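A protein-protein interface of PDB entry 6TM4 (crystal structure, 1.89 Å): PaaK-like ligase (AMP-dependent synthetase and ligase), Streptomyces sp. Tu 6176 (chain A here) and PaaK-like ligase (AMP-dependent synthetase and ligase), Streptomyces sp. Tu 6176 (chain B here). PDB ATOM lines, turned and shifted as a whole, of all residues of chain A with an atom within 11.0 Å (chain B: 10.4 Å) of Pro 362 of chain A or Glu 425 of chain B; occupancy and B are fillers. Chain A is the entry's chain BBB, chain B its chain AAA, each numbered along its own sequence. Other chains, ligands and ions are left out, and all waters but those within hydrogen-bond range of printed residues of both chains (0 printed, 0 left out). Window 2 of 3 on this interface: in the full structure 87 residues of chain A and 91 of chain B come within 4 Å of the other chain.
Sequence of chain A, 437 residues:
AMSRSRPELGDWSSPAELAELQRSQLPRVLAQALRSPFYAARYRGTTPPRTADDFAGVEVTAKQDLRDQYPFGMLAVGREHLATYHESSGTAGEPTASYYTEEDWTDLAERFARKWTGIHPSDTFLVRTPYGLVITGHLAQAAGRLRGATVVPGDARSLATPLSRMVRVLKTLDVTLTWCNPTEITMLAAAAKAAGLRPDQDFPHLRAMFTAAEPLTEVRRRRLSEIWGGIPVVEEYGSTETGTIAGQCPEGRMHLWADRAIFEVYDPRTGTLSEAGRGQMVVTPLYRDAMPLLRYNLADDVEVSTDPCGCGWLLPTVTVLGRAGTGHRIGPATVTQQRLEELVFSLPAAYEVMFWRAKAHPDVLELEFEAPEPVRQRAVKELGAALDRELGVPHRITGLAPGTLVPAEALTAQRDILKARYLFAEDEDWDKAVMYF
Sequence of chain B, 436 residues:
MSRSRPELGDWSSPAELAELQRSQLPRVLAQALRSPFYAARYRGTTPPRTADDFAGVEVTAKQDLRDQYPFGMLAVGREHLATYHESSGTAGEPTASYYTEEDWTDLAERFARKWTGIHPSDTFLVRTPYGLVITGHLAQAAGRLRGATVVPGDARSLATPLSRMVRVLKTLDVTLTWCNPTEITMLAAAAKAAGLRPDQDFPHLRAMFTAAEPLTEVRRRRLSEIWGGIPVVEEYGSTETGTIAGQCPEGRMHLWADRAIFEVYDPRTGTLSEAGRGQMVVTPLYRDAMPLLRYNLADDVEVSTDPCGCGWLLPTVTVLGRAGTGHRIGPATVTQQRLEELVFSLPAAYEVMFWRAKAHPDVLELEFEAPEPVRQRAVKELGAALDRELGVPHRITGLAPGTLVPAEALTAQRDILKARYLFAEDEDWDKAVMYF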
ATOM      1  N   HIS A 328     -22.636  36.880  24.408  1.00  0.00           N
ATOM      2  CA  HIS A 328     -23.489  35.983  23.579  1.00  0.00           C
ATOM      3  C   HIS A 328     -24.844  36.660  23.390  1.00  0.00           C
ATOM      4  O   HIS A 328     -25.517  36.897  24.390  1.00  0.00           O
ATOM      5  CB  HIS A 328     -23.638  34.593  24.217  1.00  0.00           C
ATOM      6  CG  HIS A 328     -22.424  34.142  24.962  1.00  0.00           C
ATOM      7  ND1 HIS A 328     -21.577  33.179  24.463  1.00  0.00           N
ATOM      8  CD2 HIS A 328     -21.892  34.551  26.141  1.00  0.00           C
ATOM      9  CE1 HIS A 328     -20.575  32.993  25.307  1.00  0.00           C
ATOM     10  NE2 HIS A 328     -20.746  33.825  26.353  1.00  0.00           N
ATOM     11  N   ARG A 329     -25.182  37.001  22.143  1.00  0.00           N
ATOM     12  CA  ARG A 329     -26.469  37.613  21.724  1.00  0.00           C
ATOM     13  C   ARG A 329     -27.319  36.490  21.123  1.00  0.00           C
ATOM     14  O   ARG A 329     -26.729  35.641  20.441  1.00  0.00           O
ATOM     15  CB  ARG A 329     -26.208  38.747  20.716  1.00  0.00           C
ATOM     16  CG  ARG A 329     -25.487  39.966  21.289  1.00  0.00           C
ATOM     17  CD  ARG A 329     -24.742  40.828  20.272  1.00  0.00           C
ATOM     18  NE  ARG A 329     -23.651  41.619  20.853  1.00  0.00           N
ATOM     19  CZ  ARG A 329     -22.451  41.139  21.218  1.00  0.00           C
ATOM     20  NH1 ARG A 329     -22.158  39.856  21.070  1.00  0.00           N
ATOM     21  NH2 ARG A 329     -21.540  41.944  21.744  1.00  0.00           N
ATOM     22  N   ILE A 330     -28.635  36.480  21.367  1.00  0.00           N
ATOM     23  CA  ILE A 330     -29.581  35.418  20.907  1.00  0.00           C
ATOM     24  C   ILE A 330     -30.818  36.112  20.336  1.00  0.00           C
ATOM     25  O   ILE A 330     -31.730  36.438  21.131  1.00  0.00           O
ATOM     26  CB  ILE A 330     -29.943  34.438  22.046  1.00  0.00           C
ATOM     27  CG1 ILE A 330     -28.698  33.882  22.746  1.00  0.00           C
ATOM     28  CG2 ILE A 330     -30.855  33.318  21.544  1.00  0.00           C
ATOM     29  CD1 ILE A 330     -28.997  32.763  23.736  1.00  0.00           C
ATOM     30  N   GLY A 331     -30.836  36.311  19.015  1.00  0.00           N
ATOM     31  CA  GLY A 331     -31.853  37.114  18.315  1.00  0.00           C
ATOM     32  C   GLY A 331     -31.887  38.531  18.881  1.00  0.00           C
ATOM     33  O   GLY A 331     -30.848  39.189  18.933  1.00  0.00           O
ATOM     34  N   PRO A 332     -33.054  39.012  19.380  1.00  0.00           N
ATOM     35  CA  PRO A 332     -33.191  40.403  19.822  1.00  0.00           C
ATOM     36  C   PRO A 332     -32.368  40.733  21.080  1.00  0.00           C
ATOM     37  O   PRO A 332     -31.907  41.853  21.193  1.00  0.00           O
ATOM     38  CB  PRO A 332     -34.702  40.543  20.099  1.00  0.00           C
ATOM     39  CG  PRO A 332     -35.160  39.136  20.441  1.00  0.00           C
ATOM     40  CD  PRO A 332     -34.291  38.234  19.588  1.00  0.00           C
ATOM     41  N   ALA A 333     -32.166  39.749  21.964  1.00  0.00           N
ATOM     42  CA  ALA A 333     -31.646  39.941  23.337  1.00  0.00           C
ATOM     43  C   ALA A 333     -30.141  39.671  23.407  1.00  0.00           C
ATOM     44  O   ALA A 333     -29.631  38.843  22.628  1.00  0.00           O
ATOM     45  CB  ALA A 333     -32.391  39.041  24.281  1.00  0.00           C
ATOM     46  N   THR A 334     -29.473  40.359  24.333  1.00  0.00           N
ATOM     47  CA  THR A 334     -28.064  40.131  24.738  1.00  0.00           C
ATOM     48  C   THR A 334     -28.101  39.349  26.063  1.00  0.00           C
ATOM     49  O   THR A 334     -28.701  39.853  27.021  1.00  0.00           O
ATOM     50  CB  THR A 334     -27.284  41.459  24.759  1.00  0.00           C
ATOM     51  OG1 THR A 334     -26.021  41.254  25.388  1.00  0.00           O
ATOM     52  CG2 THR A 334     -27.993  42.586  25.477  1.00  0.00           C
ATOM     53  N   VAL A 335     -27.548  38.134  26.094  1.00  0.00           N
ATOM     54  CA  VAL A 335     -27.609  37.206  27.266  1.00  0.00           C
ATOM     55  C   VAL A 335     -26.205  37.086  27.850  1.00  0.00           C
ATOM     56  O   VAL A 335     -25.315  36.620  27.119  1.00  0.00           O
ATOM     57  CB  VAL A 335     -28.152  35.827  26.847  1.00  0.00           C
ATOM     58  CG1 VAL A 335     -28.010  34.800  27.960  1.00  0.00           C
ATOM     59  CG2 VAL A 335     -29.590  35.899  26.350  1.00  0.00           C
ATOM     60  N   ALA A 358     -25.522  26.662  30.866  1.00  0.00           N
ATOM     61  CA  ALA A 358     -26.315  27.149  29.720  1.00  0.00           C
ATOM     62  C   ALA A 358     -25.434  27.227  28.479  1.00  0.00           C
ATOM     63  O   ALA A 358     -24.220  27.514  28.597  1.00  0.00           O
ATOM     64  CB  ALA A 358     -26.948  28.485  30.064  1.00  0.00           C
ATOM     65  N   LYS A 359     -26.049  27.022  27.329  1.00  0.00           N
ATOM     66  CA  LYS A 359     -25.383  27.177  26.017  1.00  0.00           C
ATOM     67  C   LYS A 359     -26.238  28.099  25.138  1.00  0.00           C
ATOM     68  O   LYS A 359     -27.469  27.849  25.025  1.00  0.00           O
ATOM     69  CB  LYS A 359     -25.212  25.791  25.396  1.00  0.00           C
ATOM     70  CG  LYS A 359     -24.274  25.722  24.205  1.00  0.00           C
ATOM     71  CD  LYS A 359     -24.079  24.308  23.731  1.00  0.00           C
ATOM     72  CE  LYS A 359     -23.203  23.481  24.650  1.00  0.00           C
ATOM     73  NZ  LYS A 359     -23.423  22.037  24.397  1.00  0.00           N
ATOM     74  N   ALA A 360     -25.608  29.128  24.561  1.00  0.00           N
ATOM     75  CA  ALA A 360     -26.202  30.034  23.546  1.00  0.00           C
ATOM     76  C   ALA A 360     -26.137  29.352  22.174  1.00  0.00           C
ATOM     77  O   ALA A 360     -25.024  29.144  21.665  1.00  0.00           O
ATOM     78  CB  ALA A 360     -25.480  31.367  23.535  1.00  0.00           C
ATOM     79  N   HIS A 361     -27.285  28.967  21.626  1.00  0.00           N
ATOM     80  CA  HIS A 361     -27.450  28.628  20.185  1.00  0.00           C
ATOM     81  C   HIS A 361     -27.898  29.902  19.468  1.00  0.00           C
ATOM     82  O   HIS A 361     -28.311  30.857  20.127  1.00  0.00           O
ATOM     83  CB  HIS A 361     -28.422  27.441  20.009  1.00  0.00           C
ATOM     84  CG  HIS A 361     -28.069  26.248  20.832  1.00  0.00           C
ATOM     85  ND1 HIS A 361     -27.169  25.290  20.402  1.00  0.00           N
ATOM     86  CD2 HIS A 361     -28.479  25.857  22.060  1.00  0.00           C
ATOM     87  CE1 HIS A 361     -27.032  24.369  21.335  1.00  0.00           C
ATOM     88  NE2 HIS A 361     -27.812  24.702  22.369  1.00  0.00           N
ATOM     89  N   PRO A 362     -27.834  29.963  18.114  1.00  0.00           N
ATOM     90  CA  PRO A 362     -28.231  31.160  17.366  1.00  0.00           C
ATOM     91  C   PRO A 362     -29.668  31.744  17.672  1.00  0.00           C
ATOM     92  O   PRO A 362     -29.892  33.025  17.485  1.00  0.00           O
ATOM     93  CB  PRO A 362     -28.202  30.678  15.898  1.00  0.00           C
ATOM     94  CG  PRO A 362     -27.165  29.575  15.886  1.00  0.00           C
ATOM     95  CD  PRO A 362     -27.323  28.897  17.230  1.00  0.00           C
ATOM     96  N   ASP A 363     -30.599  30.779  17.950  1.00  0.00           N
ATOM     97  CA  ASP A 363     -32.061  31.057  18.061  1.00  0.00           C
ATOM     98  C   ASP A 363     -32.597  30.760  19.470  1.00  0.00           C
ATOM     99  O   ASP A 363     -33.744  31.171  19.743  1.00  0.00           O
ATOM    100  CB  ASP A 363     -32.848  30.249  17.023  1.00  0.00           C
ATOM    101  CG  ASP A 363     -32.610  28.745  17.114  1.00  0.00           C
ATOM    102  OD1 ASP A 363     -31.344  28.369  17.528  1.00  0.00           O
ATOM    103  OD2 ASP A 363     -33.613  27.968  16.709  1.00  0.00           O
ATOM    104  N   VAL A 364     -31.861  30.048  20.334  1.00  0.00           N
ATOM    105  CA  VAL A 364     -32.451  29.506  21.603  1.00  0.00           C
ATOM    106  C   VAL A 364     -31.367  29.356  22.677  1.00  0.00           C
ATOM    107  O   VAL A 364     -30.208  29.030  22.344  1.00  0.00           O
ATOM    108  CB  VAL A 364     -33.224  28.194  21.330  1.00  0.00           C
ATOM    109  CG1 VAL A 364     -32.328  27.087  20.782  1.00  0.00           C
ATOM    110  CG2 VAL A 364     -34.011  27.705  22.540  1.00  0.00           C
ATOM    111  N   LEU A 365     -31.733  29.656  23.923  1.00  0.00           N
ATOM    112  CA  LEU A 365     -30.866  29.449  25.105  1.00  0.00           C
ATOM    113  C   LEU A 365     -31.247  28.098  25.726  1.00  0.00           C
ATOM    114  O   LEU A 365     -32.461  27.944  26.178  1.00  0.00           O
ATOM    115  CB  LEU A 365     -31.035  30.591  26.115  1.00  0.00           C
ATOM    116  CG  LEU A 365     -30.166  30.450  27.366  1.00  0.00           C
ATOM    117  CD1 LEU A 365     -28.705  30.705  27.027  1.00  0.00           C
ATOM    118  CD2 LEU A 365     -30.652  31.357  28.485  1.00  0.00           C
ATOM    119  N   GLU A 366     -30.276  27.152  25.697  1.00  0.00           N
ATOM    120  CA  GLU A 366     -30.415  25.844  26.388  1.00  0.00           C
ATOM    121  C   GLU A 366     -29.851  26.025  27.806  1.00  0.00           C
ATOM    122  O   GLU A 366     -28.731  26.561  27.947  1.00  0.00           O
ATOM    123  CB  GLU A 366     -29.725  24.749  25.559  1.00  0.00           C
ATOM    124  CG  GLU A 366     -29.775  23.343  26.155  1.00  0.00           C
ATOM    125  CD  GLU A 366     -28.949  22.214  25.399  1.00  0.00           C
ATOM    126  OE1 GLU A 366     -28.227  22.593  24.442  1.00  0.00           O
ATOM    127  OE2 GLU A 366     -29.146  20.930  25.721  1.00  0.00           O
ATOM    128  N   GLY A 392     -36.588  37.927  27.417  1.00  0.00           N
ATOM    129  CA  GLY A 392     -37.464  37.631  26.270  1.00  0.00           C
ATOM    130  C   GLY A 392     -36.794  36.740  25.236  1.00  0.00           C
ATOM    131  O   GLY A 392     -37.198  36.823  24.073  1.00  0.00           O
ATOM    132  N   VAL A 393     -35.811  35.915  25.624  1.00  0.00           N
ATOM    133  CA  VAL A 393     -35.140  34.945  24.696  1.00  0.00           C
ATOM    134  C   VAL A 393     -35.918  33.638  24.691  1.00  0.00           C
ATOM    135  O   VAL A 393     -36.399  33.204  25.735  1.00  0.00           O
ATOM    136  CB  VAL A 393     -33.660  34.666  25.024  1.00  0.00           C
ATOM    137  CG1 VAL A 393     -32.775  35.773  24.494  1.00  0.00           C
ATOM    138  CG2 VAL A 393     -33.407  34.421  26.507  1.00  0.00           C
ATOM    139  N   PRO A 394     -35.998  32.950  23.529  1.00  0.00           N
ATOM    140  CA  PRO A 394     -36.512  31.587  23.477  1.00  0.00           C
ATOM    141  C   PRO A 394     -35.532  30.712  24.272  1.00  0.00           C
ATOM    142  O   PRO A 394     -34.317  30.990  24.249  1.00  0.00           O
ATOM    143  CB  PRO A 394     -36.551  31.231  21.978  1.00  0.00           C
ATOM    144  CG  PRO A 394     -36.372  32.556  21.260  1.00  0.00           C
ATOM    145  CD  PRO A 394     -35.552  33.412  22.208  1.00  0.00           C
ATOM    146  N   HIS A 395     -36.069  29.724  24.990  1.00  0.00           N
ATOM    147  CA  HIS A 395     -35.303  28.899  25.957  1.00  0.00           C
ATOM    148  C   HIS A 395     -35.776  27.445  25.894  1.00  0.00           C
ATOM    149  O   HIS A 395     -36.960  27.203  25.591  1.00  0.00           O
ATOM    150  CB  HIS A 395     -35.384  29.507  27.373  1.00  0.00           C
ATOM    151  CG  HIS A 395     -36.764  29.644  27.924  1.00  0.00           C
ATOM    152  ND1 HIS A 395     -37.505  28.544  28.334  1.00  0.00           N
ATOM    153  CD2 HIS A 395     -37.539  30.735  28.131  1.00  0.00           C
ATOM    154  CE1 HIS A 395     -38.688  28.949  28.761  1.00  0.00           C
ATOM    155  NE2 HIS A 395     -38.734  30.297  28.641  1.00  0.00           N
ATOM    156  N   ARG B 420     -17.505  27.946  34.877  1.00  0.00           N
ATOM    157  CA  ARG B 420     -18.215  28.780  33.873  1.00  0.00           C
ATOM    158  C   ARG B 420     -19.627  28.223  33.742  1.00  0.00           C
ATOM    159  O   ARG B 420     -19.786  27.005  33.888  1.00  0.00           O
ATOM    160  CB  ARG B 420     -17.505  28.769  32.518  1.00  0.00           C
ATOM    161  CG  ARG B 420     -16.138  29.440  32.558  1.00  0.00           C
ATOM    162  CD  ARG B 420     -15.559  29.624  31.170  1.00  0.00           C
ATOM    163  NE  ARG B 420     -16.539  30.130  30.220  1.00  0.00           N
ATOM    164  CZ  ARG B 420     -16.616  29.764  28.939  1.00  0.00           C
ATOM    165  NH1 ARG B 420     -15.807  28.844  28.446  1.00  0.00           N
ATOM    166  NH2 ARG B 420     -17.533  30.282  28.154  1.00  0.00           N
ATOM    167  N   LEU B 422     -22.146  29.914  31.372  1.00  0.00           N
ATOM    168  CA  LEU B 422     -22.683  30.242  30.019  1.00  0.00           C
ATOM    169  C   LEU B 422     -21.623  29.890  28.971  1.00  0.00           C
ATOM    170  O   LEU B 422     -20.434  30.384  29.106  1.00  0.00           O
ATOM    171  CB  LEU B 422     -23.068  31.722  29.947  1.00  0.00           C
ATOM    172  CG  LEU B 422     -23.513  32.204  28.570  1.00  0.00           C
ATOM    173  CD1 LEU B 422     -24.707  31.399  28.075  1.00  0.00           C
ATOM    174  CD2 LEU B 422     -23.840  33.685  28.627  1.00  0.00           C
ATOM    175  N   PHE B 423     -22.026  29.057  27.984  1.00  0.00           N
ATOM    176  CA  PHE B 423     -21.103  28.533  26.947  1.00  0.00           C
ATOM    177  C   PHE B 423     -21.640  28.919  25.574  1.00  0.00           C
ATOM    178  O   PHE B 423     -22.891  29.078  25.440  1.00  0.00           O
ATOM    179  CB  PHE B 423     -20.946  27.020  27.092  1.00  0.00           C
ATOM    180  CG  PHE B 423     -20.211  26.619  28.342  1.00  0.00           C
ATOM    181  CD1 PHE B 423     -20.876  26.524  29.556  1.00  0.00           C
ATOM    182  CD2 PHE B 423     -18.850  26.391  28.312  1.00  0.00           C
ATOM    183  CE1 PHE B 423     -20.198  26.173  30.712  1.00  0.00           C
ATOM    184  CE2 PHE B 423     -18.170  26.037  29.469  1.00  0.00           C
ATOM    185  CZ  PHE B 423     -18.847  25.936  30.667  1.00  0.00           C
ATOM    186  N   ALA B 424     -20.738  29.068  24.593  1.00  0.00           N
ATOM    187  CA  ALA B 424     -21.114  29.188  23.158  1.00  0.00           C
ATOM    188  C   ALA B 424     -21.489  27.791  22.645  1.00  0.00           C
ATOM    189  O   ALA B 424     -21.094  26.795  23.283  1.00  0.00           O
ATOM    190  CB  ALA B 424     -19.987  29.800  22.355  1.00  0.00           C
ATOM    191  N   GLU B 425     -22.181  27.714  21.516  1.00  0.00           N
ATOM    192  CA  GLU B 425     -22.776  26.465  20.975  1.00  0.00           C
ATOM    193  C   GLU B 425     -21.729  25.352  20.842  1.00  0.00           C
ATOM    194  O   GLU B 425     -22.064  24.184  21.064  1.00  0.00           O
ATOM    195  CB  GLU B 425     -23.378  26.767  19.613  1.00  0.00           C
ATOM    196  CG  GLU B 425     -24.203  25.632  19.052  1.00  0.00           C
ATOM    197  CD  GLU B 425     -24.934  26.059  17.800  1.00  0.00           C
ATOM    198  OE1 GLU B 425     -26.157  25.815  17.702  1.00  0.00           O
ATOM    199  OE2 GLU B 425     -24.272  26.658  16.937  1.00  0.00           O
ATOM    200  N   ASP B 426     -20.502  25.709  20.474  1.00  0.00           N
ATOM    201  CA  ASP B 426     -19.461  24.763  20.001  1.00  0.00           C
ATOM    202  C   ASP B 426     -18.513  24.419  21.149  1.00  0.00           C
ATOM    203  O   ASP B 426     -17.583  23.634  20.889  1.00  0.00           O
ATOM    204  CB  ASP B 426     -18.709  25.345  18.799  1.00  0.00           C
ATOM    205  CG  ASP B 426     -18.626  26.863  18.822  1.00  0.00           C
ATOM    206  OD1 ASP B 426     -18.006  27.405  19.774  1.00  0.00           O
ATOM    207  OD2 ASP B 426     -19.237  27.494  17.917  1.00  0.00           O
ATOM    208  N   GLU B 427     -18.715  24.980  22.350  1.00  0.00           N
ATOM    209  CA  GLU B 427     -17.823  24.747  23.523  1.00  0.00           C
ATOM    210  C   GLU B 427     -18.309  23.529  24.320  1.00  0.00           C
ATOM    211  O   GLU B 427     -19.506  23.178  24.256  1.00  0.00           O
ATOM    212  CB  GLU B 427     -17.737  25.961  24.458  1.00  0.00           C
ATOM    213  CG  GLU B 427     -17.408  27.272  23.768  1.00  0.00           C
ATOM    214  CD  GLU B 427     -17.107  28.420  24.719  1.00  0.00           C
ATOM    215  OE1 GLU B 427     -18.054  29.102  25.164  1.00  0.00           O
ATOM    216  OE2 GLU B 427     -15.926  28.613  25.033  1.00  0.00           O
ATOM    217  N   ASP B 428     -17.389  22.940  25.073  1.00  0.00           N
ATOM    218  CA  ASP B 428     -17.640  21.803  25.985  1.00  0.00           C
ATOM    219  C   ASP B 428     -18.243  22.363  27.273  1.00  0.00           C
ATOM    220  O   ASP B 428     -17.454  22.927  28.081  1.00  0.00           O
ATOM    221  CB  ASP B 428     -16.326  21.078  26.286  1.00  0.00           C
ATOM    222  CG  ASP B 428     -16.482  19.839  27.147  1.00  0.00           C
ATOM    223  OD1 ASP B 428     -17.599  19.254  27.157  1.00  0.00           O
ATOM    224  OD2 ASP B 428     -15.455  19.429  27.741  1.00  0.00           O
ATOM    225  N   TRP B 429     -19.561  22.219  27.492  1.00  0.00           N
ATOM    226  CA  TRP B 429     -20.172  22.703  28.763  1.00  0.00           C
ATOM    227  C   TRP B 429     -20.030  21.664  29.884  1.00  0.00           C
ATOM    228  O   TRP B 429     -20.477  21.958  31.004  1.00  0.00           O
ATOM    229  CB  TRP B 429     -21.605  23.193  28.583  1.00  0.00           C
ATOM    230  CG  TRP B 429     -22.644  22.145  28.342  1.00  0.00           C
ATOM    231  CD1 TRP B 429     -22.452  20.838  27.990  1.00  0.00           C
ATOM    232  CD2 TRP B 429     -24.062  22.345  28.400  1.00  0.00           C
ATOM    233  NE1 TRP B 429     -23.661  20.215  27.841  1.00  0.00           N
ATOM    234  CE2 TRP B 429     -24.667  21.113  28.065  1.00  0.00           C
ATOM    235  CE3 TRP B 429     -24.885  23.442  28.676  1.00  0.00           C
ATOM    236  CZ2 TRP B 429     -26.047  20.941  28.028  1.00  0.00           C
ATOM    237  CZ3 TRP B 429     -26.251  23.271  28.636  1.00  0.00           C
ATOM    238  CH2 TRP B 429     -26.826  22.042  28.294  1.00  0.00           C
ATOM    239  N   ASP B 430     -19.348  20.541  29.640  1.00  0.00           N
ATOM    240  CA  ASP B 430     -19.050  19.548  30.707  1.00  0.00           C
ATOM    241  C   ASP B 430     -18.088  20.149  31.745  1.00  0.00           C
ATOM    242  O   ASP B 430     -18.042  19.608  32.858  1.00  0.00           O
ATOM    243  CB  ASP B 430     -18.549  18.226  30.120  1.00  0.00           C
ATOM    244  CG  ASP B 430     -19.688  17.407  29.524  1.00  0.00           C
ATOM    245  OD1 ASP B 430     -20.848  17.791  29.708  1.00  0.00           O
ATOM    246  OD2 ASP B 430     -19.399  16.403  28.884  1.00  0.00           O
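Among the printed residues, pairs that only touch across the chains: His 328 of chain A with Leu 422 of chain B, His 328 of chain A with Ala 424 of chain B, Val 335 of chain A with Leu 422 of chain B, Ala 358 of chain A with Leu 422 of chain B, Ala 358 of chain A with Trp 429 of chain B, Lys 359 of chain A with Phe 423 of chain B, Lys 359 of chain A with Ala 424 of chain B, Lys 359 of chain A with Glu 425 of chain B, Lys 359 of chain A with Glu 427 of chain B, Lys 359 of chain A with Trp 429 of chain B, Ala 360 of chain A with Ala 424 of chain B, Pro 362 of chain A with Glu 425 of chain B and Glu 366 of chain A with Trp 429 of chain B.
The backbone NH (N) of Glu 425 of chain B sits at hydrogen-bond distance from the backbone carbonyl oxygen (O) of Ala 360 of chain A (3.2 Å). N of Phe 423 of chain B is in hydrogen-bond range of O of Ala 358 of chain A (2.8 Å). The backbone NH (N) of Ala 360 of chain A is in hydrogen-bond range of the backbone carbonyl oxygen (O) of Phe 423 of chain B (2.9 Å). OE1 of Glu 425 of chain B sits at hydrogen-bond distance from ND1 of His 361 of chain A, 2.9 Å away.
No residue of chain B comes within 4 Å of Ile 330 of chain A. Of the printed residues of chain B, Ala 358 of chain A touches Leu 422, Phe 423 and Trp 429. Printed residues of chain B within 4 Å of Lys 359 of chain A: Phe 423, Ala 424, Glu 425, Glu 427 and Trp 429. Ala 360 of chain A touches just these residues of chain B: Phe 423, Ala 424 and Glu 425. His 361 of chain A touches one residue of chain B. Pro 362 of chain A touches one residue of chain B. Of the printed residues of chain B, Glu 366 of chain A touches Trp 429. Glu 425 of chain B touches just these residues of chain A: Lys 359, Ala 360, His 361 and Pro 362. No residue of chain A comes within 4 Å of Asp 426 of chain B. The nearest residue of chain B that does not touch Pro 362 of chain A is Ala 424 of chain B (8.0 Å). The nearest residue of chain A that does not touch Glu 425 of chain B is Asp 363 of chain A (5.8 Å).
Of the 21 printed residues of chain A, 8 touch a printed residue of chain B. Printed residues of chain A that touch a printed residue of chain B: His 328, Val 335, Ala 358, Lys 359, Ala 360, His 361, Pro 362 and Glu 366. Hydrophobic or aromatic side chains of chain B within 4 Å of the printed part of chain A: Leu 422, Phe 423 and Trp 429. Among the printed residues, no Asp or Glu carboxylate lies within 4 Å of a Lys or Arg side-chain nitrogen of the other chain.
The backbone carbonyl oxygen (O) of Glu 366 of chain A lies within hydrogen-bond range of the backbone NH (N) of Lys 359 of chain A (2.8 Å). The side-chain carboxylate of Glu 427 of chain B is in hydrogen-bond range of the backbone NH of Ala 424 of chain B, at 2.7 Å. NH2 of Arg 420 of chain B sits at hydrogen-bond distance from O of Leu 422 of chain B, 3.1 Å away. The backbone carbonyl oxygen of His 328 of chain A is in hydrogen-bond range of the backbone NH of Val 335 of chain A (2.9 Å). The guanidinium group of Arg 420 of chain B is in salt-bridge range of the side-chain carboxylate of Glu 427 of chain B (3.3 Å). OE1 of Glu 366 of chain A is in hydrogen-bond range of NE2 of His 361 of chain A, 3.0 Å away.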
